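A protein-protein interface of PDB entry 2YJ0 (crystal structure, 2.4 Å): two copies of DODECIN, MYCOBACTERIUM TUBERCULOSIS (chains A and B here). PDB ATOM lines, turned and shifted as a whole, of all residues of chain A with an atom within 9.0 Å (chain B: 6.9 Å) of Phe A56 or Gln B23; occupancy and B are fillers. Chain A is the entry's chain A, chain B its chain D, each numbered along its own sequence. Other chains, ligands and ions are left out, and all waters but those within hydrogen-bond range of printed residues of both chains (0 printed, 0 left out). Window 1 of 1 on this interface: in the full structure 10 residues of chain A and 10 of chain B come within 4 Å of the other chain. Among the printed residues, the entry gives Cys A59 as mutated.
OD1 of Asp B19 is in hydrogen-bond range of N of Val A18.
The backbone carbonyl oxygen of Gly A46 sits at hydrogen-bond distance from the backbone NH of Phe B39.
The backbone carbonyl oxygen (O) of Ser A14 sits at hydrogen-bond distance from the backbone NH (N) of Phe A56, at 2.6 Å.
N of Arg A45 is in hydrogen-bond range of O of Gln A57, 2.7 Å away.
Among the printed residues, merely in contact across the chains: Val A53 with Leu B26 (3.2 Å), Arg A45 with Phe B39 (3.3 Å), Gly A17 with Asp B19 (3.5 Å), Phe A56 with Gln B23 (3.5 Å), Phe A56 with Asp B19 (3.9 Å), Leu A48 with Leu B26 (3.9 Å), Leu A48 with Phe B39 (3.96 Å) and Val A53 with Phe B39 (3.97 Å).
Phe A56 touches just these residues of chain B: Asp B19 and Gln B23.
Gln B23 touches one residue of chain A.
Gly B24 touches none of the printed residues of chain A.
Printed residues of chain B within 4 Å of Val A53: Leu B26 and Phe B39.
Printed residues of chain A within 4 Å of Leu B26: Leu A48 (3.9 Å) and Val A53 (3.2 Å).
Hydrophobic or aromatic side chains of chain B that line the printed part of chain A: Leu B26 and Phe B39.
Among the printed residues, no Asp or Glu carboxylate lies within 4 Å of a Lys or Arg side-chain nitrogen of the other chain.
Val A18 touches Asp B19, but with the chains exchanged Asp A19 does not touch Val B18 (7.0 Å).
Of the 10 pairs that touch across the chains among the printed residues, none has its exchanged pair printed and touching as well.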
ATOM      1  N   VAL A  11      21.244   6.943 -15.005  1.00  0.00           N
ATOM      2  CA  VAL A  11      21.138   6.615 -16.425  1.00  0.00           C
ATOM      3  C   VAL A  11      21.935   7.630 -17.234  1.00  0.00           C
ATOM      4  O   VAL A  11      21.588   8.810 -17.283  1.00  0.00           O
ATOM      5  CB  VAL A  11      19.679   6.601 -16.929  1.00  0.00           C
ATOM      6  CG1 VAL A  11      19.634   6.146 -18.382  1.00  0.00           C
ATOM      7  CG2 VAL A  11      18.820   5.688 -16.070  1.00  0.00           C
ATOM      8  N   GLY A  12      23.016   7.163 -17.850  1.00  0.00           N
ATOM      9  CA  GLY A  12      23.793   7.989 -18.761  1.00  0.00           C
ATOM     10  C   GLY A  12      23.162   7.967 -20.139  1.00  0.00           C
ATOM     11  O   GLY A  12      22.597   6.948 -20.548  1.00  0.00           O
ATOM     12  N   THR A  13      23.237   9.089 -20.852  1.00  0.00           N
ATOM     13  CA  THR A  13      22.715   9.151 -22.218  1.00  0.00           C
ATOM     14  C   THR A  13      23.725   9.723 -23.216  1.00  0.00           C
ATOM     15  O   THR A  13      24.617  10.495 -22.859  1.00  0.00           O
ATOM     16  CB  THR A  13      21.387   9.952 -22.305  1.00  0.00           C
ATOM     17  OG1 THR A  13      21.648  11.350 -22.152  1.00  0.00           O
ATOM     18  CG2 THR A  13      20.394   9.492 -21.236  1.00  0.00           C
ATOM     19  N   SER A  14      23.562   9.309 -24.470  1.00  0.00           N
ATOM     20  CA  SER A  14      24.371   9.774 -25.589  1.00  0.00           C
ATOM     21  C   SER A  14      23.628   9.488 -26.881  1.00  0.00           C
ATOM     22  O   SER A  14      22.936   8.478 -26.976  1.00  0.00           O
ATOM     23  CB  SER A  14      25.725   9.064 -25.624  1.00  0.00           C
ATOM     24  OG  SER A  14      26.400   9.317 -26.851  1.00  0.00           O
ATOM     25  N   PRO A  15      23.765  10.370 -27.884  1.00  0.00           N
ATOM     26  CA  PRO A  15      23.252  10.037 -29.207  1.00  0.00           C
ATOM     27  C   PRO A  15      24.179   9.133 -30.033  1.00  0.00           C
ATOM     28  O   PRO A  15      23.777   8.691 -31.105  1.00  0.00           O
ATOM     29  CB  PRO A  15      23.103  11.406 -29.878  1.00  0.00           C
ATOM     30  CG  PRO A  15      24.079  12.267 -29.206  1.00  0.00           C
ATOM     31  CD  PRO A  15      24.202  11.772 -27.802  1.00  0.00           C
ATOM     32  N   ASP A  16      25.389   8.854 -29.541  1.00  0.00           N
ATOM     33  CA  ASP A  16      26.389   8.092 -30.311  1.00  0.00           C
ATOM     34  C   ASP A  16      26.369   6.593 -30.052  1.00  0.00           C
ATOM     35  O   ASP A  16      26.463   5.799 -30.988  1.00  0.00           O
ATOM     36  CB  ASP A  16      27.797   8.624 -30.038  1.00  0.00           C
ATOM     37  CG  ASP A  16      27.994  10.018 -30.568  1.00  0.00           C
ATOM     38  OD1 ASP A  16      26.979  10.710 -30.789  1.00  0.00           O
ATOM     39  OD2 ASP A  16      29.159  10.420 -30.766  1.00  0.00           O
ATOM     40  N   GLY A  17      26.268   6.199 -28.790  1.00  0.00           N
ATOM     41  CA  GLY A  17      26.264   4.778 -28.475  1.00  0.00           C
ATOM     42  C   GLY A  17      26.290   4.423 -27.008  1.00  0.00           C
ATOM     43  O   GLY A  17      26.191   5.288 -26.135  1.00  0.00           O
ATOM     44  N   VAL A  18      26.443   3.128 -26.754  1.00  0.00           N
ATOM     45  CA  VAL A  18      26.405   2.581 -25.403  1.00  0.00           C
ATOM     46  C   VAL A  18      27.584   3.055 -24.556  1.00  0.00           C
ATOM     47  O   VAL A  18      27.403   3.427 -23.395  1.00  0.00           O
ATOM     48  CB  VAL A  18      26.377   1.032 -25.429  1.00  0.00           C
ATOM     49  CG1 VAL A  18      26.538   0.462 -24.025  1.00  0.00           C
ATOM     50  CG2 VAL A  18      25.083   0.541 -26.057  1.00  0.00           C
ATOM     51  N   ASP A  19      28.781   3.048 -25.136  1.00  0.00           N
ATOM     52  CA  ASP A  19      29.987   3.436 -24.398  1.00  0.00           C
ATOM     53  C   ASP A  19      29.930   4.911 -24.017  1.00  0.00           C
ATOM     54  O   ASP A  19      30.258   5.278 -22.888  1.00  0.00           O
ATOM     55  CB  ASP A  19      31.257   3.155 -25.210  1.00  0.00           C
ATOM     56  CG  ASP A  19      31.362   1.706 -25.650  1.00  0.00           C
ATOM     57  OD1 ASP A  19      31.356   0.814 -24.780  1.00  0.00           O
ATOM     58  OD2 ASP A  19      31.453   1.456 -26.872  1.00  0.00           O
ATOM     59  N   ALA A  20      29.504   5.744 -24.964  1.00  0.00           N
ATOM     60  CA  ALA A  20      29.396   7.183 -24.745  1.00  0.00           C
ATOM     61  C   ALA A  20      28.332   7.530 -23.698  1.00  0.00           C
ATOM     62  O   ALA A  20      28.479   8.507 -22.956  1.00  0.00           O
ATOM     63  CB  ALA A  20      29.097   7.897 -26.061  1.00  0.00           C
ATOM     64  N   ALA A  21      27.261   6.740 -23.653  1.00  0.00           N
ATOM     65  CA  ALA A  21      26.208   6.922 -22.657  1.00  0.00           C
ATOM     66  C   ALA A  21      26.747   6.600 -21.269  1.00  0.00           C
ATOM     67  O   ALA A  21      26.593   7.391 -20.336  1.00  0.00           O
ATOM     68  CB  ALA A  21      25.009   6.044 -22.982  1.00  0.00           C
ATOM     69  N   ILE A  22      27.386   5.438 -21.150  1.00  0.00           N
ATOM     70  CA  ILE A  22      28.051   5.024 -19.916  1.00  0.00           C
ATOM     71  C   ILE A  22      28.967   6.123 -19.402  1.00  0.00           C
ATOM     72  O   ILE A  22      28.864   6.550 -18.249  1.00  0.00           O
ATOM     73  CB  ILE A  22      28.906   3.757 -20.132  1.00  0.00           C
ATOM     74  CG1 ILE A  22      28.017   2.515 -20.216  1.00  0.00           C
ATOM     75  CG2 ILE A  22      29.928   3.598 -19.006  1.00  0.00           C
ATOM     76  CD1 ILE A  22      28.739   1.290 -20.764  1.00  0.00           C
ATOM     77  N   GLY A  24      29.177   9.294 -20.422  1.00  0.00           N
ATOM     78  CA  GLY A  24      28.396  10.497 -20.173  1.00  0.00           C
ATOM     79  C   GLY A  24      27.811  10.504 -18.774  1.00  0.00           C
ATOM     80  O   GLY A  24      27.939  11.490 -18.048  1.00  0.00           O
ATOM     81  N   GLY A  25      27.187   9.392 -18.391  1.00  0.00           N
ATOM     82  CA  GLY A  25      26.580   9.255 -17.066  1.00  0.00           C
ATOM     83  C   GLY A  25      27.588   9.307 -15.929  1.00  0.00           C
ATOM     84  O   GLY A  25      27.354   9.971 -14.919  1.00  0.00           O
ATOM     85  N   SER A  43      20.492  -1.948 -17.600  1.00  0.00           N
ATOM     86  CA  SER A  43      19.809  -2.087 -18.880  1.00  0.00           C
ATOM     87  C   SER A  43      20.319  -1.100 -19.913  1.00  0.00           C
ATOM     88  O   SER A  43      20.855  -0.043 -19.577  1.00  0.00           O
ATOM     89  CB  SER A  43      18.298  -1.906 -18.714  1.00  0.00           C
ATOM     90  OG  SER A  43      17.984  -0.562 -18.399  1.00  0.00           O
ATOM     91  N   ILE A  44      20.140  -1.476 -21.175  1.00  0.00           N
ATOM     92  CA  ILE A  44      20.435  -0.619 -22.305  1.00  0.00           C
ATOM     93  C   ILE A  44      19.123  -0.356 -23.032  1.00  0.00           C
ATOM     94  O   ILE A  44      18.421  -1.290 -23.431  1.00  0.00           O
ATOM     95  CB  ILE A  44      21.441  -1.275 -23.261  1.00  0.00           C
ATOM     96  CG1 ILE A  44      22.723  -1.649 -22.509  1.00  0.00           C
ATOM     97  CG2 ILE A  44      21.757  -0.332 -24.422  1.00  0.00           C
ATOM     98  CD1 ILE A  44      23.642  -2.563 -23.281  1.00  0.00           C
ATOM     99  N   ARG A  45      18.804   0.923 -23.192  1.00  0.00           N
ATOM    100  CA  ARG A  45      17.552   1.363 -23.783  1.00  0.00           C
ATOM    101  C   ARG A  45      17.807   2.523 -24.731  1.00  0.00           C
ATOM    102  O   ARG A  45      18.937   2.979 -24.875  1.00  0.00           O
ATOM    103  CB  ARG A  45      16.591   1.812 -22.684  1.00  0.00           C
ATOM    104  CG  ARG A  45      15.825   0.686 -22.048  1.00  0.00           C
ATOM    105  CD  ARG A  45      15.266   1.099 -20.702  1.00  0.00           C
ATOM    106  NE  ARG A  45      14.418   0.055 -20.132  1.00  0.00           N
ATOM    107  CZ  ARG A  45      13.140  -0.149 -20.444  1.00  0.00           C
ATOM    108  NH1 ARG A  45      12.514   0.611 -21.337  1.00  0.00           N
ATOM    109  NH2 ARG A  45      12.476  -1.133 -19.858  1.00  0.00           N
ATOM    110  N   GLY A  46      16.750   2.993 -25.381  1.00  0.00           N
ATOM    111  CA  GLY A  46      16.845   4.196 -26.187  1.00  0.00           C
ATOM    112  C   GLY A  46      15.512   4.742 -26.645  1.00  0.00           C
ATOM    113  O   GLY A  46      14.519   4.024 -26.716  1.00  0.00           O
ATOM    114  N   HIS A  47      15.515   6.034 -26.952  1.00  0.00           N
ATOM    115  CA  HIS A  47      14.348   6.742 -27.451  1.00  0.00           C
ATOM    116  C   HIS A  47      14.511   6.877 -28.957  1.00  0.00           C
ATOM    117  O   HIS A  47      15.609   7.167 -29.442  1.00  0.00           O
ATOM    118  CB  HIS A  47      14.268   8.117 -26.782  1.00  0.00           C
ATOM    119  CG  HIS A  47      13.102   8.949 -27.217  1.00  0.00           C
ATOM    120  ND1 HIS A  47      11.809   8.474 -27.240  1.00  0.00           N
ATOM    121  CD2 HIS A  47      13.035  10.241 -27.617  1.00  0.00           C
ATOM    122  CE1 HIS A  47      10.996   9.431 -27.652  1.00  0.00           C
ATOM    123  NE2 HIS A  47      11.716  10.514 -27.888  1.00  0.00           N
ATOM    124  N   LEU A  48      13.424   6.662 -29.691  1.00  0.00           N
ATOM    125  CA  LEU A  48      13.453   6.709 -31.147  1.00  0.00           C
ATOM    126  C   LEU A  48      12.642   7.894 -31.664  1.00  0.00           C
ATOM    127  O   LEU A  48      11.464   8.040 -31.335  1.00  0.00           O
ATOM    128  CB  LEU A  48      12.922   5.397 -31.727  1.00  0.00           C
ATOM    129  CG  LEU A  48      13.630   4.146 -31.192  1.00  0.00           C
ATOM    130  CD1 LEU A  48      12.970   2.876 -31.696  1.00  0.00           C
ATOM    131  CD2 LEU A  48      15.114   4.168 -31.555  1.00  0.00           C
ATOM    132  N   GLY A  51      12.183   7.146 -36.510  1.00  0.00           N
ATOM    133  CA  GLY A  51      12.813   5.853 -36.805  1.00  0.00           C
ATOM    134  C   GLY A  51      14.281   5.685 -36.429  1.00  0.00           C
ATOM    135  O   GLY A  51      14.882   4.655 -36.746  1.00  0.00           O
ATOM    136  N   ALA A  52      14.856   6.674 -35.742  1.00  0.00           N
ATOM    137  CA  ALA A  52      16.291   6.695 -35.439  1.00  0.00           C
ATOM    138  C   ALA A  52      16.545   6.822 -33.941  1.00  0.00           C
ATOM    139  O   ALA A  52      15.763   7.444 -33.229  1.00  0.00           O
ATOM    140  CB  ALA A  52      16.947   7.851 -36.164  1.00  0.00           C
ATOM    141  N   VAL A  53      17.654   6.257 -33.470  1.00  0.00           N
ATOM    142  CA  VAL A  53      18.013   6.352 -32.057  1.00  0.00           C
ATOM    143  C   VAL A  53      18.416   7.786 -31.724  1.00  0.00           C
ATOM    144  O   VAL A  53      19.480   8.244 -32.136  1.00  0.00           O
ATOM    145  CB  VAL A  53      19.174   5.401 -31.686  1.00  0.00           C
ATOM    146  CG1 VAL A  53      19.478   5.489 -30.194  1.00  0.00           C
ATOM    147  CG2 VAL A  53      18.846   3.973 -32.075  1.00  0.00           C
ATOM    148  N   ALA A  54      17.562   8.497 -30.993  1.00  0.00           N
ATOM    149  CA  ALA A  54      17.851   9.884 -30.612  1.00  0.00           C
ATOM    150  C   ALA A  54      18.842   9.908 -29.458  1.00  0.00           C
ATOM    151  O   ALA A  54      19.805  10.679 -29.468  1.00  0.00           O
ATOM    152  CB  ALA A  54      16.574  10.622 -30.234  1.00  0.00           C
ATOM    153  N   HIS A  55      18.593   9.063 -28.463  1.00  0.00           N
ATOM    154  CA  HIS A  55      19.514   8.879 -27.349  1.00  0.00           C
ATOM    155  C   HIS A  55      19.628   7.413 -26.981  1.00  0.00           C
ATOM    156  O   HIS A  55      18.617   6.735 -26.813  1.00  0.00           O
ATOM    157  CB  HIS A  55      19.040   9.653 -26.120  1.00  0.00           C
ATOM    158  CG  HIS A  55      19.106  11.135 -26.281  1.00  0.00           C
ATOM    159  ND1 HIS A  55      20.224  11.871 -25.950  1.00  0.00           N
ATOM    160  CD2 HIS A  55      18.194  12.022 -26.740  1.00  0.00           C
ATOM    161  CE1 HIS A  55      19.994  13.148 -26.197  1.00  0.00           C
ATOM    162  NE2 HIS A  55      18.769  13.266 -26.676  1.00  0.00           N
ATOM    163  N   PHE A  56      20.863   6.936 -26.877  1.00  0.00           N
ATOM    164  CA  PHE A  56      21.162   5.683 -26.201  1.00  0.00           C
ATOM    165  C   PHE A  56      21.058   5.954 -24.703  1.00  0.00           C
ATOM    166  O   PHE A  56      21.500   7.004 -24.234  1.00  0.00           O
ATOM    167  CB  PHE A  56      22.570   5.190 -26.555  1.00  0.00           C
ATOM    168  CG  PHE A  56      22.703   4.687 -27.969  1.00  0.00           C
ATOM    169  CD1 PHE A  56      22.857   5.573 -29.030  1.00  0.00           C
ATOM    170  CD2 PHE A  56      22.669   3.327 -28.239  1.00  0.00           C
ATOM    171  CE1 PHE A  56      22.973   5.107 -30.335  1.00  0.00           C
ATOM    172  CE2 PHE A  56      22.786   2.855 -29.539  1.00  0.00           C
ATOM    173  CZ  PHE A  56      22.937   3.744 -30.588  1.00  0.00           C
ATOM    174  N   GLN A  57      20.464   5.021 -23.961  1.00  0.00           N
ATOM    175  CA  GLN A  57      20.247   5.186 -22.525  1.00  0.00           C
ATOM    176  C   GLN A  57      20.722   3.950 -21.778  1.00  0.00           C
ATOM    177  O   GLN A  57      20.198   2.857 -21.992  1.00  0.00           O
ATOM    178  CB  GLN A  57      18.764   5.411 -22.237  1.00  0.00           C
ATOM    179  CG  GLN A  57      18.201   6.711 -22.796  1.00  0.00           C
ATOM    180  CD  GLN A  57      16.688   6.681 -22.958  1.00  0.00           C
ATOM    181  OE1 GLN A  57      16.059   5.622 -22.881  1.00  0.00           O
ATOM    182  NE2 GLN A  57      16.099   7.849 -23.190  1.00  0.00           N
ATOM    183  N   VAL A  58      21.706   4.132 -20.900  1.00  0.00           N
ATOM    184  CA  VAL A  58      22.296   3.027 -20.160  1.00  0.00           C
ATOM    185  C   VAL A  58      22.130   3.239 -18.667  1.00  0.00           C
ATOM    186  O   VAL A  58      22.790   4.092 -18.067  1.00  0.00           O
ATOM    187  CB  VAL A  58      23.787   2.874 -20.480  1.00  0.00           C
ATOM    188  CG1 VAL A  58      24.375   1.695 -19.713  1.00  0.00           C
ATOM    189  CG2 VAL A  58      23.988   2.708 -21.980  1.00  0.00           C
ATOM    190  N   CYS A  59      21.238   2.454 -18.075  1.00  0.00           N
ATOM    191  CA  CYS A  59      21.004   2.500 -16.645  1.00  0.00           C
ATOM    192  C   CYS A  59      22.110   1.727 -15.932  1.00  0.00           C
ATOM    193  O   CYS A  59      22.365   0.563 -16.246  1.00  0.00           O
ATOM    194  CB  CYS A  59      19.634   1.916 -16.315  1.00  0.00           C
ATOM    195  SG  CYS A  59      19.241   1.888 -14.557  1.00  0.00           S
ATOM    196  N   GLY B  12      19.021  -7.337 -34.237  1.00  0.00           N
ATOM    197  CA  GLY B  12      19.873  -6.630 -35.192  1.00  0.00           C
ATOM    198  C   GLY B  12      21.209  -7.342 -35.257  1.00  0.00           C
ATOM    199  O   GLY B  12      21.628  -7.955 -34.275  1.00  0.00           O
ATOM    200  N   VAL B  18      28.337  -3.684 -31.168  1.00  0.00           N
ATOM    201  CA  VAL B  18      27.032  -3.714 -30.510  1.00  0.00           C
ATOM    202  C   VAL B  18      26.127  -2.576 -30.991  1.00  0.00           C
ATOM    203  O   VAL B  18      24.954  -2.804 -31.291  1.00  0.00           O
ATOM    204  CB  VAL B  18      27.183  -3.660 -28.978  1.00  0.00           C
ATOM    205  CG1 VAL B  18      25.825  -3.592 -28.304  1.00  0.00           C
ATOM    206  CG2 VAL B  18      27.956  -4.874 -28.491  1.00  0.00           C
ATOM    207  N   ASP B  19      26.672  -1.362 -31.067  1.00  0.00           N
ATOM    208  CA  ASP B  19      25.914  -0.202 -31.543  1.00  0.00           C
ATOM    209  C   ASP B  19      25.437  -0.414 -32.978  1.00  0.00           C
ATOM    210  O   ASP B  19      24.273  -0.180 -33.298  1.00  0.00           O
ATOM    211  CB  ASP B  19      26.763   1.070 -31.481  1.00  0.00           C
ATOM    212  CG  ASP B  19      27.079   1.502 -30.062  1.00  0.00           C
ATOM    213  OD1 ASP B  19      26.276   1.224 -29.148  1.00  0.00           O
ATOM    214  OD2 ASP B  19      28.135   2.138 -29.866  1.00  0.00           O
ATOM    215  N   ALA B  20      26.355  -0.856 -33.831  1.00  0.00           N
ATOM    216  CA  ALA B  20      26.068  -1.129 -35.238  1.00  0.00           C
ATOM    217  C   ALA B  20      24.957  -2.162 -35.405  1.00  0.00           C
ATOM    218  O   ALA B  20      24.099  -2.026 -36.272  1.00  0.00           O
ATOM    219  CB  ALA B  20      27.333  -1.604 -35.941  1.00  0.00           C
ATOM    220  N   ALA B  21      24.988  -3.195 -34.569  1.00  0.00           N
ATOM    221  CA  ALA B  21      23.947  -4.218 -34.561  1.00  0.00           C
ATOM    222  C   ALA B  21      22.610  -3.622 -34.144  1.00  0.00           C
ATOM    223  O   ALA B  21      21.586  -3.924 -34.746  1.00  0.00           O
ATOM    224  CB  ALA B  21      24.330  -5.362 -33.630  1.00  0.00           C
ATOM    225  N   ILE B  22      22.620  -2.777 -33.114  1.00  0.00           N
ATOM    226  CA  ILE B  22      21.391  -2.126 -32.651  1.00  0.00           C
ATOM    227  C   ILE B  22      20.788  -1.267 -33.752  1.00  0.00           C
ATOM    228  O   ILE B  22      19.601  -1.379 -34.045  1.00  0.00           O
ATOM    229  CB  ILE B  22      21.624  -1.241 -31.403  1.00  0.00           C
ATOM    230  CG1 ILE B  22      21.886  -2.105 -30.170  1.00  0.00           C
ATOM    231  CG2 ILE B  22      20.416  -0.351 -31.143  1.00  0.00           C
ATOM    232  CD1 ILE B  22      22.502  -1.331 -29.015  1.00  0.00           C
ATOM    233  N   GLN B  23      21.613  -0.425 -34.369  1.00  0.00           N
ATOM    234  CA  GLN B  23      21.126   0.525 -35.372  1.00  0.00           C
ATOM    235  C   GLN B  23      20.684  -0.136 -36.685  1.00  0.00           C
ATOM    236  O   GLN B  23      19.793   0.378 -37.368  1.00  0.00           O
ATOM    237  CB  GLN B  23      22.161   1.634 -35.622  1.00  0.00           C
ATOM    238  CG  GLN B  23      21.855   2.926 -34.840  1.00  0.00           C
ATOM    239  CD  GLN B  23      23.092   3.680 -34.388  1.00  0.00           C
ATOM    240  OE1 GLN B  23      24.212   3.163 -34.438  1.00  0.00           O
ATOM    241  NE2 GLN B  23      22.893   4.910 -33.928  1.00  0.00           N
ATOM    242  N   GLY B  24      21.291  -1.274 -37.020  1.00  0.00           N
ATOM    243  CA  GLY B  24      20.917  -2.033 -38.215  1.00  0.00           C
ATOM    244  C   GLY B  24      19.577  -2.728 -38.057  1.00  0.00           C
ATOM    245  O   GLY B  24      18.788  -2.807 -39.002  1.00  0.00           O
ATOM    246  N   GLY B  25      19.321  -3.241 -36.858  1.00  0.00           N
ATOM    247  CA  GLY B  25      18.040  -3.861 -36.551  1.00  0.00           C
ATOM    248  C   GLY B  25      16.924  -2.836 -36.531  1.00  0.00           C
ATOM    249  O   GLY B  25      15.865  -3.049 -37.120  1.00  0.00           O
ATOM    250  N   LEU B  26      17.168  -1.718 -35.851  1.00  0.00           N
ATOM    251  CA  LEU B  26      16.194  -0.634 -35.787  1.00  0.00           C
ATOM    252  C   LEU B  26      15.903  -0.057 -37.174  1.00  0.00           C
ATOM    253  O   LEU B  26      14.755   0.257 -37.484  1.00  0.00           O
ATOM    254  CB  LEU B  26      16.674   0.463 -34.831  1.00  0.00           C
ATOM    255  CG  LEU B  26      16.757   0.037 -33.359  1.00  0.00           C
ATOM    256  CD1 LEU B  26      17.419   1.108 -32.515  1.00  0.00           C
ATOM    257  CD2 LEU B  26      15.383  -0.295 -32.813  1.00  0.00           C
ATOM    258  N   ALA B  27      16.938   0.060 -38.006  1.00  0.00           N
ATOM    259  CA  ALA B  27      16.791   0.585 -39.370  1.00  0.00           C
ATOM    260  C   ALA B  27      15.855  -0.264 -40.235  1.00  0.00           C
ATOM    261  O   ALA B  27      15.108   0.273 -41.054  1.00  0.00           O
ATOM    262  CB  ALA B  27      18.161   0.710 -40.047  1.00  0.00           C
ATOM    263  N   ARG B  28      15.903  -1.583 -40.059  1.00  0.00           N
ATOM    264  CA  ARG B  28      15.009  -2.479 -40.790  1.00  0.00           C
ATOM    265  C   ARG B  28      13.575  -2.313 -40.294  1.00  0.00           C
ATOM    266  O   ARG B  28      12.629  -2.431 -41.070  1.00  0.00           O
ATOM    267  CB  ARG B  28      15.461  -3.940 -40.656  1.00  0.00           C
ATOM    268  CG  ARG B  28      14.507  -4.976 -41.271  1.00  0.00           C
ATOM    269  CD  ARG B  28      14.224  -4.717 -42.748  1.00  0.00           C
ATOM    270  NE  ARG B  28      13.302  -5.698 -43.322  1.00  0.00           N
ATOM    271  CZ  ARG B  28      11.979  -5.700 -43.157  1.00  0.00           C
ATOM    272  NH1 ARG B  28      11.375  -4.773 -42.418  1.00  0.00           N
ATOM    273  NH2 ARG B  28      11.249  -6.649 -43.733  1.00  0.00           N
ATOM    274  N   PHE B  39      13.427   1.327 -27.598  1.00  0.00           N
ATOM    275  CA  PHE B  39      13.895  -0.048 -27.626  1.00  0.00           C
ATOM    276  C   PHE B  39      14.528  -0.414 -26.291  1.00  0.00           C
ATOM    277  O   PHE B  39      14.916   0.464 -25.513  1.00  0.00           O
ATOM    278  CB  PHE B  39      14.885  -0.276 -28.778  1.00  0.00           C
ATOM    279  CG  PHE B  39      16.254   0.290 -28.531  1.00  0.00           C
ATOM    280  CD1 PHE B  39      17.228  -0.462 -27.882  1.00  0.00           C
ATOM    281  CD2 PHE B  39      16.574   1.572 -28.952  1.00  0.00           C
ATOM    282  CE1 PHE B  39      18.494   0.058 -27.650  1.00  0.00           C
ATOM    283  CE2 PHE B  39      17.845   2.098 -28.725  1.00  0.00           C
ATOM    284  CZ  PHE B  39      18.803   1.338 -28.071  1.00  0.00           C
ATOM    285  N   MET B  60      16.508  -7.120 -29.383  1.00  0.00           N
ATOM    286  CA  MET B  60      15.846  -5.906 -28.917  1.00  0.00           C
ATOM    287  C   MET B  60      14.333  -6.039 -28.883  1.00  0.00           C
ATOM    288  O   MET B  60      13.725  -6.561 -29.817  1.00  0.00           O
ATOM    289  CB  MET B  60      16.182  -4.737 -29.845  1.00  0.00           C
ATOM    290  CG  MET B  60      17.633  -4.332 -29.873  1.00  0.00           C
ATOM    291  SD  MET B  60      17.899  -2.988 -31.045  1.00  0.00           S
ATOM    292  CE  MET B  60      17.760  -3.862 -32.605  1.00  0.00           C
